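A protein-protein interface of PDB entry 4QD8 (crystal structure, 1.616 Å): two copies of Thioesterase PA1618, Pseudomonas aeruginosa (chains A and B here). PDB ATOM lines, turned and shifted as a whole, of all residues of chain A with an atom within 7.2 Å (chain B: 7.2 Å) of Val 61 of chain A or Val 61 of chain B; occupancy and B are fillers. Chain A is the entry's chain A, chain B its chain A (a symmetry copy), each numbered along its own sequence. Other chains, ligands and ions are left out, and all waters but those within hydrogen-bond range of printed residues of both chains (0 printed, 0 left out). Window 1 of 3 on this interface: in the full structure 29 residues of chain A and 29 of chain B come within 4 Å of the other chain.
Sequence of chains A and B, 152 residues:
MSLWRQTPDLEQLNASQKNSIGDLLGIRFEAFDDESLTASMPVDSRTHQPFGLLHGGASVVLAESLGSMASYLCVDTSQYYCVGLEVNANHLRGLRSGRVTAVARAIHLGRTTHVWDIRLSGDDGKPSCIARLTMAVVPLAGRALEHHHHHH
Hydrophobic or aromatic side chains of chain A within 4 Å of the printed part of chain B: Ile 21, Leu 25, His 55, Ala 58, Val 60 and Val 61.
Of the 18 printed residues of chain B, 10 touch a printed residue of chain A.
Hydrophobic or aromatic side chains of chain B within 4 Å of the printed part of chain A: Ile 21, Leu 25, His 55, Ala 58, Val 60 and Val 61.
Among the printed residues, 22 pairs touch across the chains.
Among the printed residues, no Asp or Glu carboxylate lies within 4 Å of a Lys or Arg side-chain nitrogen of the other chain.
Among the printed residues, merely in contact across the chains: Ile 21 of chain A with Leu 25 of chain B, Ile 21 of chain A with His 55 of chain B, Ile 21 of chain A with Ala 58 of chain B, Leu 25 of chain A with Ile 21 of chain B, His 55 of chain A with Ile 21 of chain B, His 55 of chain A with Val 61 of chain B, His 55 of chain A with Glu 64 of chain B, Gly 56 of chain A with Glu 64 of chain B, Gly 57 of chain A with Val 61 of chain B, Gly 57 of chain A with Glu 64 of chain B, Ala 58 of chain A with Ile 21 of chain B, Ala 58 of chain A with Val 61 of chain B, Val 60 of chain A with Val 60 of chain B, Val 61 of chain A with His 55 of chain B, Val 61 of chain A with Gly 57 of chain B, Val 61 of chain A with Ala 58 of chain B, Val 61 of chain A with Val 61 of chain B, Glu 64 of chain A with His 55 of chain B, Glu 64 of chain A with Gly 56 of chain B and Glu 64 of chain A with Gly 57 of chain B.
His 55 of chain A touches Val 61 of chain B, and with the chains exchanged Val 61 of chain A touches His 55 of chain B.
His 55 of chain A touches Ser 65 of chain B, and with the chains exchanged Ser 65 of chain A touches His 55 of chain B.
Gly 57 of chain A touches Glu 64 of chain B, and with the chains exchanged Glu 64 of chain A touches Gly 57 of chain B.
Val 60 of chain B touches its own counterpart, Val 60 of chain A.
Of the 22 pairs that touch across the chains among the printed residues, 22 have their exchanged pair printed and touching as well.
Val 61 of chain A touches just these residues of chain B: His 55, Gly 57, Ala 58 and Val 61.
Of the printed residues of chain A, Ile 21 of chain B touches Leu 25 (3.98 Å), His 55 (3.2 Å) and Ala 58 (3.997 Å).
Printed residues of chain A within 4 Å of His 55 of chain B: Ile 21, Val 61, Glu 64 and Ser 65.
Of the printed residues of chain A, Gly 56 of chain B touches Glu 64 (3.3 Å).
Val 61 of chain B touches four residues of chain A.
The nearest printed residue of chain B that does not touch Glu 64 of chain A is Val 60 of chain B (5.4 Å).
A ring nitrogen (NE2) of His 55 of chain B is in hydrogen-bond range of the side-chain hydroxyl (OG) of Ser 65 of chain A (2.8 Å).
NE2 of His 55 of chain A sits at hydrogen-bond distance from OG of Ser 65 of chain B (2.8 Å).
ND1 of His 55 of chain A sits at hydrogen-bond distance from N of Gly 57 of chain A, at 2.9 Å.
The side-chain hydroxyl of Ser 65 of chain A lies close to the backbone carbonyl oxygen of Val 61 of chain A (3.4 Å).
ND1 of His 55 of chain B lies within hydrogen-bond range of N of Gly 57 of chain B.
The backbone carbonyl oxygen (O) of Val 61 of chain B sits close to the side-chain hydroxyl (OG) of Ser 65 of chain B, at 3.4 Å.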
ATOM      1  N   ILE A  21      24.035 -16.396  11.797  1.00  0.00           N
ATOM      2  CA  ILE A  21      24.034 -17.248  12.990  1.00  0.00           C
ATOM      3  C   ILE A  21      25.268 -18.145  13.080  1.00  0.00           C
ATOM      4  O   ILE A  21      25.753 -18.456  14.184  1.00  0.00           O
ATOM      5  CB  ILE A  21      22.722 -18.072  13.084  1.00  0.00           C
ATOM      6  CG1 ILE A  21      22.594 -18.758  14.457  1.00  0.00           C
ATOM      7  CG2 ILE A  21      22.620 -19.062  11.930  1.00  0.00           C
ATOM      8  CD1 ILE A  21      21.234 -19.393  14.680  1.00  0.00           C
ATOM      9  N   GLY A  22      25.792 -18.568  11.934  1.00  0.00           N
ATOM     10  CA  GLY A  22      26.948 -19.452  11.934  1.00  0.00           C
ATOM     11  C   GLY A  22      28.157 -18.823  12.610  1.00  0.00           C
ATOM     12  O   GLY A  22      28.906 -19.489  13.335  1.00  0.00           O
ATOM     13  N   LEU A  25      27.498 -18.669  16.445  1.00  0.00           N
ATOM     14  CA  LEU A  25      27.654 -19.940  17.160  1.00  0.00           C
ATOM     15  C   LEU A  25      29.037 -20.571  17.037  1.00  0.00           C
ATOM     16  O   LEU A  25      29.278 -21.629  17.603  1.00  0.00           O
ATOM     17  CB  LEU A  25      26.591 -20.944  16.706  1.00  0.00           C
ATOM     18  CG  LEU A  25      25.134 -20.498  16.827  1.00  0.00           C
ATOM     19  CD1 LEU A  25      24.230 -21.658  16.417  1.00  0.00           C
ATOM     20  CD2 LEU A  25      24.831 -20.033  18.252  1.00  0.00           C
ATOM     21  N   ILE A  27      30.446 -21.784  14.248  1.00  0.00           N
ATOM     22  CA  ILE A  27      30.555 -22.811  13.217  1.00  0.00           C
ATOM     23  C   ILE A  27      31.795 -22.574  12.360  1.00  0.00           C
ATOM     24  O   ILE A  27      32.058 -21.457  11.898  1.00  0.00           O
ATOM     25  CB  ILE A  27      29.276 -22.897  12.348  1.00  0.00           C
ATOM     26  CG1 ILE A  27      28.096 -23.377  13.195  1.00  0.00           C
ATOM     27  CG2 ILE A  27      29.494 -23.842  11.155  1.00  0.00           C
ATOM     28  CD1 ILE A  27      26.728 -23.382  12.449  1.00  0.00           C
ATOM     29  N   MET A  41      31.341 -27.218  15.550  1.00  0.00           N
ATOM     30  CA  MET A  41      30.723 -26.158  16.323  1.00  0.00           C
ATOM     31  C   MET A  41      31.028 -26.422  17.782  1.00  0.00           C
ATOM     32  O   MET A  41      31.008 -27.567  18.210  1.00  0.00           O
ATOM     33  CB  MET A  41      29.211 -26.198  16.109  1.00  0.00           C
ATOM     34  CG  MET A  41      28.424 -25.036  16.714  1.00  0.00           C
ATOM     35  SD  MET A  41      26.662 -25.161  16.333  1.00  0.00           S
ATOM     36  CE  MET A  41      26.284 -26.734  17.092  1.00  0.00           C
ATOM     37  N   HIS A  55      21.932 -28.013  22.638  1.00  0.00           N
ATOM     38  CA  HIS A  55      20.540 -27.834  22.207  1.00  0.00           C
ATOM     39  C   HIS A  55      20.345 -28.586  20.894  1.00  0.00           C
ATOM     40  O   HIS A  55      21.150 -28.446  19.986  1.00  0.00           O
ATOM     41  CB  HIS A  55      20.291 -26.325  21.999  1.00  0.00           C
ATOM     42  CG  HIS A  55      18.861 -25.922  21.838  1.00  0.00           C
ATOM     43  ND1 HIS A  55      18.057 -26.351  20.797  1.00  0.00           N
ATOM     44  CD2 HIS A  55      18.107 -25.036  22.538  1.00  0.00           C
ATOM     45  CE1 HIS A  55      16.877 -25.775  20.884  1.00  0.00           C
ATOM     46  NE2 HIS A  55      16.878 -24.966  21.928  1.00  0.00           N
ATOM     47  N   GLY A  56      19.291 -29.396  20.805  1.00  0.00           N
ATOM     48  CA  GLY A  56      19.058 -30.189  19.609  1.00  0.00           C
ATOM     49  C   GLY A  56      18.857 -29.319  18.387  1.00  0.00           C
ATOM     50  O   GLY A  56      19.221 -29.697  17.273  1.00  0.00           O
ATOM     51  N   GLY A  57      18.299 -28.137  18.584  1.00  0.00           N
ATOM     52  CA  GLY A  57      18.187 -27.193  17.479  1.00  0.00           C
ATOM     53  C   GLY A  57      19.534 -26.691  16.993  1.00  0.00           C
ATOM     54  O   GLY A  57      19.721 -26.422  15.802  1.00  0.00           O
ATOM     55  N   ALA A  58      20.486 -26.545  17.907  1.00  0.00           N
ATOM     56  CA  ALA A  58      21.830 -26.116  17.521  1.00  0.00           C
ATOM     57  C   ALA A  58      22.487 -27.169  16.621  1.00  0.00           C
ATOM     58  O   ALA A  58      23.202 -26.823  15.667  1.00  0.00           O
ATOM     59  CB  ALA A  58      22.685 -25.827  18.762  1.00  0.00           C
ATOM     60  N   SER A  59      22.249 -28.448  16.905  1.00  0.00           N
ATOM     61  CA  SER A  59      22.723 -29.512  16.023  1.00  0.00           C
ATOM     62  C   SER A  59      22.141 -29.320  14.635  1.00  0.00           C
ATOM     63  O   SER A  59      22.836 -29.522  13.633  1.00  0.00           O
ATOM     64  CB  SER A  59      22.337 -30.899  16.536  1.00  0.00           C
ATOM     65  OG  SER A  59      23.171 -31.282  17.614  1.00  0.00           O
ATOM     66  N   VAL A  60      20.878 -28.913  14.579  1.00  0.00           N
ATOM     67  CA  VAL A  60      20.219 -28.713  13.293  1.00  0.00           C
ATOM     68  C   VAL A  60      20.758 -27.454  12.581  1.00  0.00           C
ATOM     69  O   VAL A  60      20.938 -27.472  11.364  1.00  0.00           O
ATOM     70  CB  VAL A  60      18.680 -28.738  13.416  1.00  0.00           C
ATOM     71  CG1 VAL A  60      18.022 -28.489  12.042  1.00  0.00           C
ATOM     72  CG2 VAL A  60      18.223 -30.097  13.963  1.00  0.00           C
ATOM     73  N   VAL A  61      21.068 -26.390  13.325  1.00  0.00           N
ATOM     74  CA  VAL A  61      21.716 -25.222  12.703  1.00  0.00           C
ATOM     75  C   VAL A  61      23.023 -25.648  12.027  1.00  0.00           C
ATOM     76  O   VAL A  61      23.297 -25.275  10.880  1.00  0.00           O
ATOM     77  CB  VAL A  61      22.039 -24.099  13.720  1.00  0.00           C
ATOM     78  CG1 VAL A  61      22.809 -22.959  13.020  1.00  0.00           C
ATOM     79  CG2 VAL A  61      20.769 -23.551  14.343  1.00  0.00           C
ATOM     80  N   LEU A  62      23.836 -26.426  12.733  1.00  0.00           N
ATOM     81  CA  LEU A  62      25.075 -26.918  12.146  1.00  0.00           C
ATOM     82  C   LEU A  62      24.795 -27.732  10.879  1.00  0.00           C
ATOM     83  O   LEU A  62      25.409 -27.500   9.829  1.00  0.00           O
ATOM     84  CB  LEU A  62      25.856 -27.751  13.156  1.00  0.00           C
ATOM     85  CG  LEU A  62      27.157 -28.363  12.641  1.00  0.00           C
ATOM     86  CD1 LEU A  62      28.071 -27.287  12.044  1.00  0.00           C
ATOM     87  CD2 LEU A  62      27.849 -29.105  13.797  1.00  0.00           C
ATOM     88  N   ALA A  63      23.837 -28.648  10.965  1.00  0.00           N
ATOM     89  CA  ALA A  63      23.522 -29.517   9.829  1.00  0.00           C
ATOM     90  C   ALA A  63      23.035 -28.704   8.642  1.00  0.00           C
ATOM     91  O   ALA A  63      23.461 -28.938   7.497  1.00  0.00           O
ATOM     92  CB  ALA A  63      22.479 -30.557  10.227  1.00  0.00           C
ATOM     93  N   GLU A  64      22.152 -27.746   8.906  1.00  0.00           N
ATOM     94  CA  GLU A  64      21.565 -26.955   7.818  1.00  0.00           C
ATOM     95  C   GLU A  64      22.569 -25.953   7.240  1.00  0.00           C
ATOM     96  O   GLU A  64      22.559 -25.702   6.032  1.00  0.00           O
ATOM     97  CB  GLU A  64      20.242 -26.286   8.239  1.00  0.00           C
ATOM     98  CG  GLU A  64      19.499 -25.692   7.052  1.00  0.00           C
ATOM     99  CD  GLU A  64      17.972 -25.698   7.175  1.00  0.00           C
ATOM    100  OE1 GLU A  64      17.380 -26.490   7.964  1.00  0.00           O
ATOM    101  OE2 GLU A  64      17.378 -24.904   6.431  1.00  0.00           O
ATOM    102  N   SER A  65      23.453 -25.407   8.078  1.00  0.00           N
ATOM    103  CA  SER A  65      24.534 -24.548   7.584  1.00  0.00           C
ATOM    104  C   SER A  65      25.416 -25.332   6.633  1.00  0.00           C
ATOM    105  O   SER A  65      25.769 -24.851   5.558  1.00  0.00           O
ATOM    106  CB  SER A  65      25.424 -24.041   8.731  1.00  0.00           C
ATOM    107  OG  SER A  65      24.936 -22.828   9.266  1.00  0.00           O
ATOM    108  N   LEU A  66      25.776 -26.536   7.055  1.00  0.00           N
ATOM    109  CA  LEU A  66      26.696 -27.379   6.321  1.00  0.00           C
ATOM    110  C   LEU A  66      26.072 -27.824   5.010  1.00  0.00           C
ATOM    111  O   LEU A  66      26.665 -27.663   3.953  1.00  0.00           O
ATOM    112  CB  LEU A  66      27.085 -28.594   7.173  1.00  0.00           C
ATOM    113  CG  LEU A  66      28.041 -29.584   6.522  1.00  0.00           C
ATOM    114  CD1 LEU A  66      29.292 -28.857   6.027  1.00  0.00           C
ATOM    115  CD2 LEU A  66      28.414 -30.661   7.518  1.00  0.00           C
ATOM    116  N   GLY A  67      24.859 -28.365   5.070  1.00  0.00           N
ATOM    117  CA  GLY A  67      24.194 -28.824   3.862  1.00  0.00           C
ATOM    118  C   GLY A  67      23.835 -27.713   2.893  1.00  0.00           C
ATOM    119  O   GLY A  67      23.897 -27.916   1.673  1.00  0.00           O
ATOM    120  N   ILE B  21      21.479 -21.006  24.357  1.00  0.00           N
ATOM    121  CA  ILE B  21      21.282 -20.455  23.013  1.00  0.00           C
ATOM    122  C   ILE B  21      20.019 -19.600  22.902  1.00  0.00           C
ATOM    123  O   ILE B  21      19.976 -18.622  22.133  1.00  0.00           O
ATOM    124  CB  ILE B  21      21.305 -21.579  21.942  1.00  0.00           C
ATOM    125  CG1 ILE B  21      21.369 -20.990  20.520  1.00  0.00           C
ATOM    126  CG2 ILE B  21      20.126 -22.526  22.124  1.00  0.00           C
ATOM    127  CD1 ILE B  21      21.614 -22.039  19.452  1.00  0.00           C
ATOM    128  N   GLY B  22      18.985 -19.948  23.661  1.00  0.00           N
ATOM    129  CA  GLY B  22      17.737 -19.205  23.590  1.00  0.00           C
ATOM    130  C   GLY B  22      17.912 -17.741  23.964  1.00  0.00           C
ATOM    131  O   GLY B  22      17.315 -16.846  23.354  1.00  0.00           O
ATOM    132  N   LEU B  25      19.857 -15.952  21.105  1.00  0.00           N
ATOM    133  CA  LEU B  25      19.068 -15.638  19.909  1.00  0.00           C
ATOM    134  C   LEU B  25      17.859 -14.744  20.165  1.00  0.00           C
ATOM    135  O   LEU B  25      17.136 -14.414  19.234  1.00  0.00           O
ATOM    136  CB  LEU B  25      18.615 -16.925  19.214  1.00  0.00           C
ATOM    137  CG  LEU B  25      19.714 -17.912  18.821  1.00  0.00           C
ATOM    138  CD1 LEU B  25      19.080 -19.077  18.064  1.00  0.00           C
ATOM    139  CD2 LEU B  25      20.784 -17.218  17.978  1.00  0.00           C
ATOM    140  N   ILE B  27      15.134 -15.520  21.955  1.00  0.00           N
ATOM    141  CA  ILE B  27      13.872 -16.235  22.112  1.00  0.00           C
ATOM    142  C   ILE B  27      13.123 -15.729  23.342  1.00  0.00           C
ATOM    143  O   ILE B  27      13.690 -15.593  24.432  1.00  0.00           O
ATOM    144  CB  ILE B  27      14.079 -17.769  22.169  1.00  0.00           C
ATOM    145  CG1 ILE B  27      14.604 -18.279  20.825  1.00  0.00           C
ATOM    146  CG2 ILE B  27      12.765 -18.480  22.531  1.00  0.00           C
ATOM    147  CD1 ILE B  27      14.966 -19.794  20.808  1.00  0.00           C
ATOM    148  N   MET B  41      10.958 -15.044  18.166  1.00  0.00           N
ATOM    149  CA  MET B  41      12.390 -14.875  18.010  1.00  0.00           C
ATOM    150  C   MET B  41      12.610 -13.817  16.949  1.00  0.00           C
ATOM    151  O   MET B  41      11.890 -13.790  15.960  1.00  0.00           O
ATOM    152  CB  MET B  41      13.003 -16.193  17.542  1.00  0.00           C
ATOM    153  CG  MET B  41      14.530 -16.236  17.498  1.00  0.00           C
ATOM    154  SD  MET B  41      15.132 -17.866  16.999  1.00  0.00           S
ATOM    155  CE  MET B  41      14.380 -18.001  15.384  1.00  0.00           C
ATOM    156  N   HIS B  55      17.654 -18.350   9.021  1.00  0.00           N
ATOM    157  CA  HIS B  55      18.295 -19.664   8.882  1.00  0.00           C
ATOM    158  C   HIS B  55      17.284 -20.734   9.280  1.00  0.00           C
ATOM    159  O   HIS B  55      16.650 -20.617  10.318  1.00  0.00           O
ATOM    160  CB  HIS B  55      19.515 -19.705   9.826  1.00  0.00           C
ATOM    161  CG  HIS B  55      20.457 -20.847   9.617  1.00  0.00           C
ATOM    162  ND1 HIS B  55      20.099 -22.173   9.777  1.00  0.00           N
ATOM    163  CD2 HIS B  55      21.788 -20.858   9.355  1.00  0.00           C
ATOM    164  CE1 HIS B  55      21.153 -22.940   9.594  1.00  0.00           C
ATOM    165  NE2 HIS B  55      22.196 -22.170   9.342  1.00  0.00           N
ATOM    166  N   GLY B  56      17.123 -21.762   8.448  1.00  0.00           N
ATOM    167  CA  GLY B  56      16.144 -22.799   8.725  1.00  0.00           C
ATOM    168  C   GLY B  56      16.442 -23.523  10.021  1.00  0.00           C
ATOM    169  O   GLY B  56      15.533 -23.970  10.721  1.00  0.00           O
ATOM    170  N   GLY B  57      17.713 -23.626  10.365  1.00  0.00           N
ATOM    171  CA  GLY B  57      18.073 -24.197  11.657  1.00  0.00           C
ATOM    172  C   GLY B  57      17.626 -23.338  12.826  1.00  0.00           C
ATOM    173  O   GLY B  57      17.279 -23.849  13.895  1.00  0.00           O
ATOM    174  N   ALA B  58      17.641 -22.023  12.646  1.00  0.00           N
ATOM    175  CA  ALA B  58      17.178 -21.120  13.699  1.00  0.00           C
ATOM    176  C   ALA B  58      15.683 -21.334  13.964  1.00  0.00           C
ATOM    177  O   ALA B  58      15.235 -21.277  15.121  1.00  0.00           O
ATOM    178  CB  ALA B  58      17.481 -19.660  13.335  1.00  0.00           C
ATOM    179  N   SER B  59      14.907 -21.587  12.911  1.00  0.00           N
ATOM    180  CA  SER B  59      13.499 -21.935  13.085  1.00  0.00           C
ATOM    181  C   SER B  59      13.384 -23.180  13.944  1.00  0.00           C
ATOM    182  O   SER B  59      12.497 -23.268  14.801  1.00  0.00           O
ATOM    183  CB  SER B  59      12.800 -22.187  11.749  1.00  0.00           C
ATOM    184  OG  SER B  59      12.522 -20.965  11.093  1.00  0.00           O
ATOM    185  N   VAL B  60      14.290 -24.127  13.729  1.00  0.00           N
ATOM    186  CA  VAL B  60      14.258 -25.370  14.491  1.00  0.00           C
ATOM    187  C   VAL B  60      14.705 -25.140  15.951  1.00  0.00           C
ATOM    188  O   VAL B  60      14.126 -25.725  16.865  1.00  0.00           O
ATOM    189  CB  VAL B  60      15.028 -26.507  13.786  1.00  0.00           C
ATOM    190  CG1 VAL B  60      15.001 -27.794  14.640  1.00  0.00           C
ATOM    191  CG2 VAL B  60      14.400 -26.790  12.415  1.00  0.00           C
ATOM    192  N   VAL B  61      15.682 -24.260  16.183  1.00  0.00           N
ATOM    193  CA  VAL B  61      16.039 -23.907  17.567  1.00  0.00           C
ATOM    194  C   VAL B  61      14.811 -23.363  18.303  1.00  0.00           C
ATOM    195  O   VAL B  61      14.520 -23.761  19.437  1.00  0.00           O
ATOM    196  CB  VAL B  61      17.163 -22.844  17.648  1.00  0.00           C
ATOM    197  CG1 VAL B  61      17.411 -22.447  19.118  1.00  0.00           C
ATOM    198  CG2 VAL B  61      18.449 -23.367  17.037  1.00  0.00           C
ATOM    199  N   LEU B  62      14.087 -22.450  17.665  1.00  0.00           N
ATOM    200  CA  LEU B  62      12.874 -21.918  18.272  1.00  0.00           C
ATOM    201  C   LEU B  62      11.873 -23.040  18.567  1.00  0.00           C
ATOM    202  O   LEU B  62      11.347 -23.140  19.684  1.00  0.00           O
ATOM    203  CB  LEU B  62      12.242 -20.860  17.374  1.00  0.00           C
ATOM    204  CG  LEU B  62      10.934 -20.260  17.883  1.00  0.00           C
ATOM    205  CD1 LEU B  62      11.102 -19.700  19.301  1.00  0.00           C
ATOM    206  CD2 LEU B  62      10.474 -19.167  16.903  1.00  0.00           C
ATOM    207  N   ALA B  63      11.651 -23.908  17.587  1.00  0.00           N
ATOM    208  CA  ALA B  63      10.676 -24.989  17.744  1.00  0.00           C
ATOM    209  C   ALA B  63      11.081 -25.926  18.869  1.00  0.00           C
ATOM    210  O   ALA B  63      10.242 -26.315  19.702  1.00  0.00           O
ATOM    211  CB  ALA B  63      10.521 -25.761  16.437  1.00  0.00           C
ATOM    212  N   GLU B  64      12.360 -26.285  18.905  1.00  0.00           N
ATOM    213  CA  GLU B  64      12.835 -27.245  19.908  1.00  0.00           C
ATOM    214  C   GLU B  64      12.909 -26.618  21.303  1.00  0.00           C
ATOM    215  O   GLU B  64      12.636 -27.297  22.297  1.00  0.00           O
ATOM    216  CB  GLU B  64      14.162 -27.908  19.490  1.00  0.00           C
ATOM    217  CG  GLU B  64      14.519 -29.086  20.384  1.00  0.00           C
ATOM    218  CD  GLU B  64      15.298 -30.209  19.695  1.00  0.00           C
ATOM    219  OE1 GLU B  64      15.273 -30.351  18.438  1.00  0.00           O
ATOM    220  OE2 GLU B  64      15.914 -30.971  20.455  1.00  0.00           O
ATOM    221  N   SER B  65      13.240 -25.327  21.387  1.00  0.00           N
ATOM    222  CA  SER B  65      13.199 -24.617  22.669  1.00  0.00           C
ATOM    223  C   SER B  65      11.786 -24.634  23.218  1.00  0.00           C
ATOM    224  O   SER B  65      11.570 -24.907  24.396  1.00  0.00           O
ATOM    225  CB  SER B  65      13.618 -23.145  22.514  1.00  0.00           C
ATOM    226  OG  SER B  65      15.013 -22.986  22.668  1.00  0.00           O
ATOM    227  N   LEU B  66      10.835 -24.323  22.348  1.00  0.00           N
ATOM    228  CA  LEU B  66       9.443 -24.193  22.724  1.00  0.00           C
ATOM    229  C   LEU B  66       8.880 -25.543  23.135  1.00  0.00           C
ATOM    230  O   LEU B  66       8.305 -25.676  24.205  1.00  0.00           O
ATOM    231  CB  LEU B  66       8.639 -23.606  21.557  1.00  0.00           C
ATOM    232  CG  LEU B  66       7.147 -23.426  21.802  1.00  0.00           C
ATOM    233  CD1 LEU B  66       6.919 -22.606  23.072  1.00  0.00           C
ATOM    234  CD2 LEU B  66       6.516 -22.740  20.609  1.00  0.00           C
ATOM    235  N   GLY B  67       9.064 -26.556  22.295  1.00  0.00           N
ATOM    236  CA  GLY B  67       8.550 -27.879  22.609  1.00  0.00           C
ATOM    237  C   GLY B  67       9.213 -28.531  23.808  1.00  0.00           C
ATOM    238  O   GLY B  67       8.544 -29.245  24.568  1.00  0.00           O
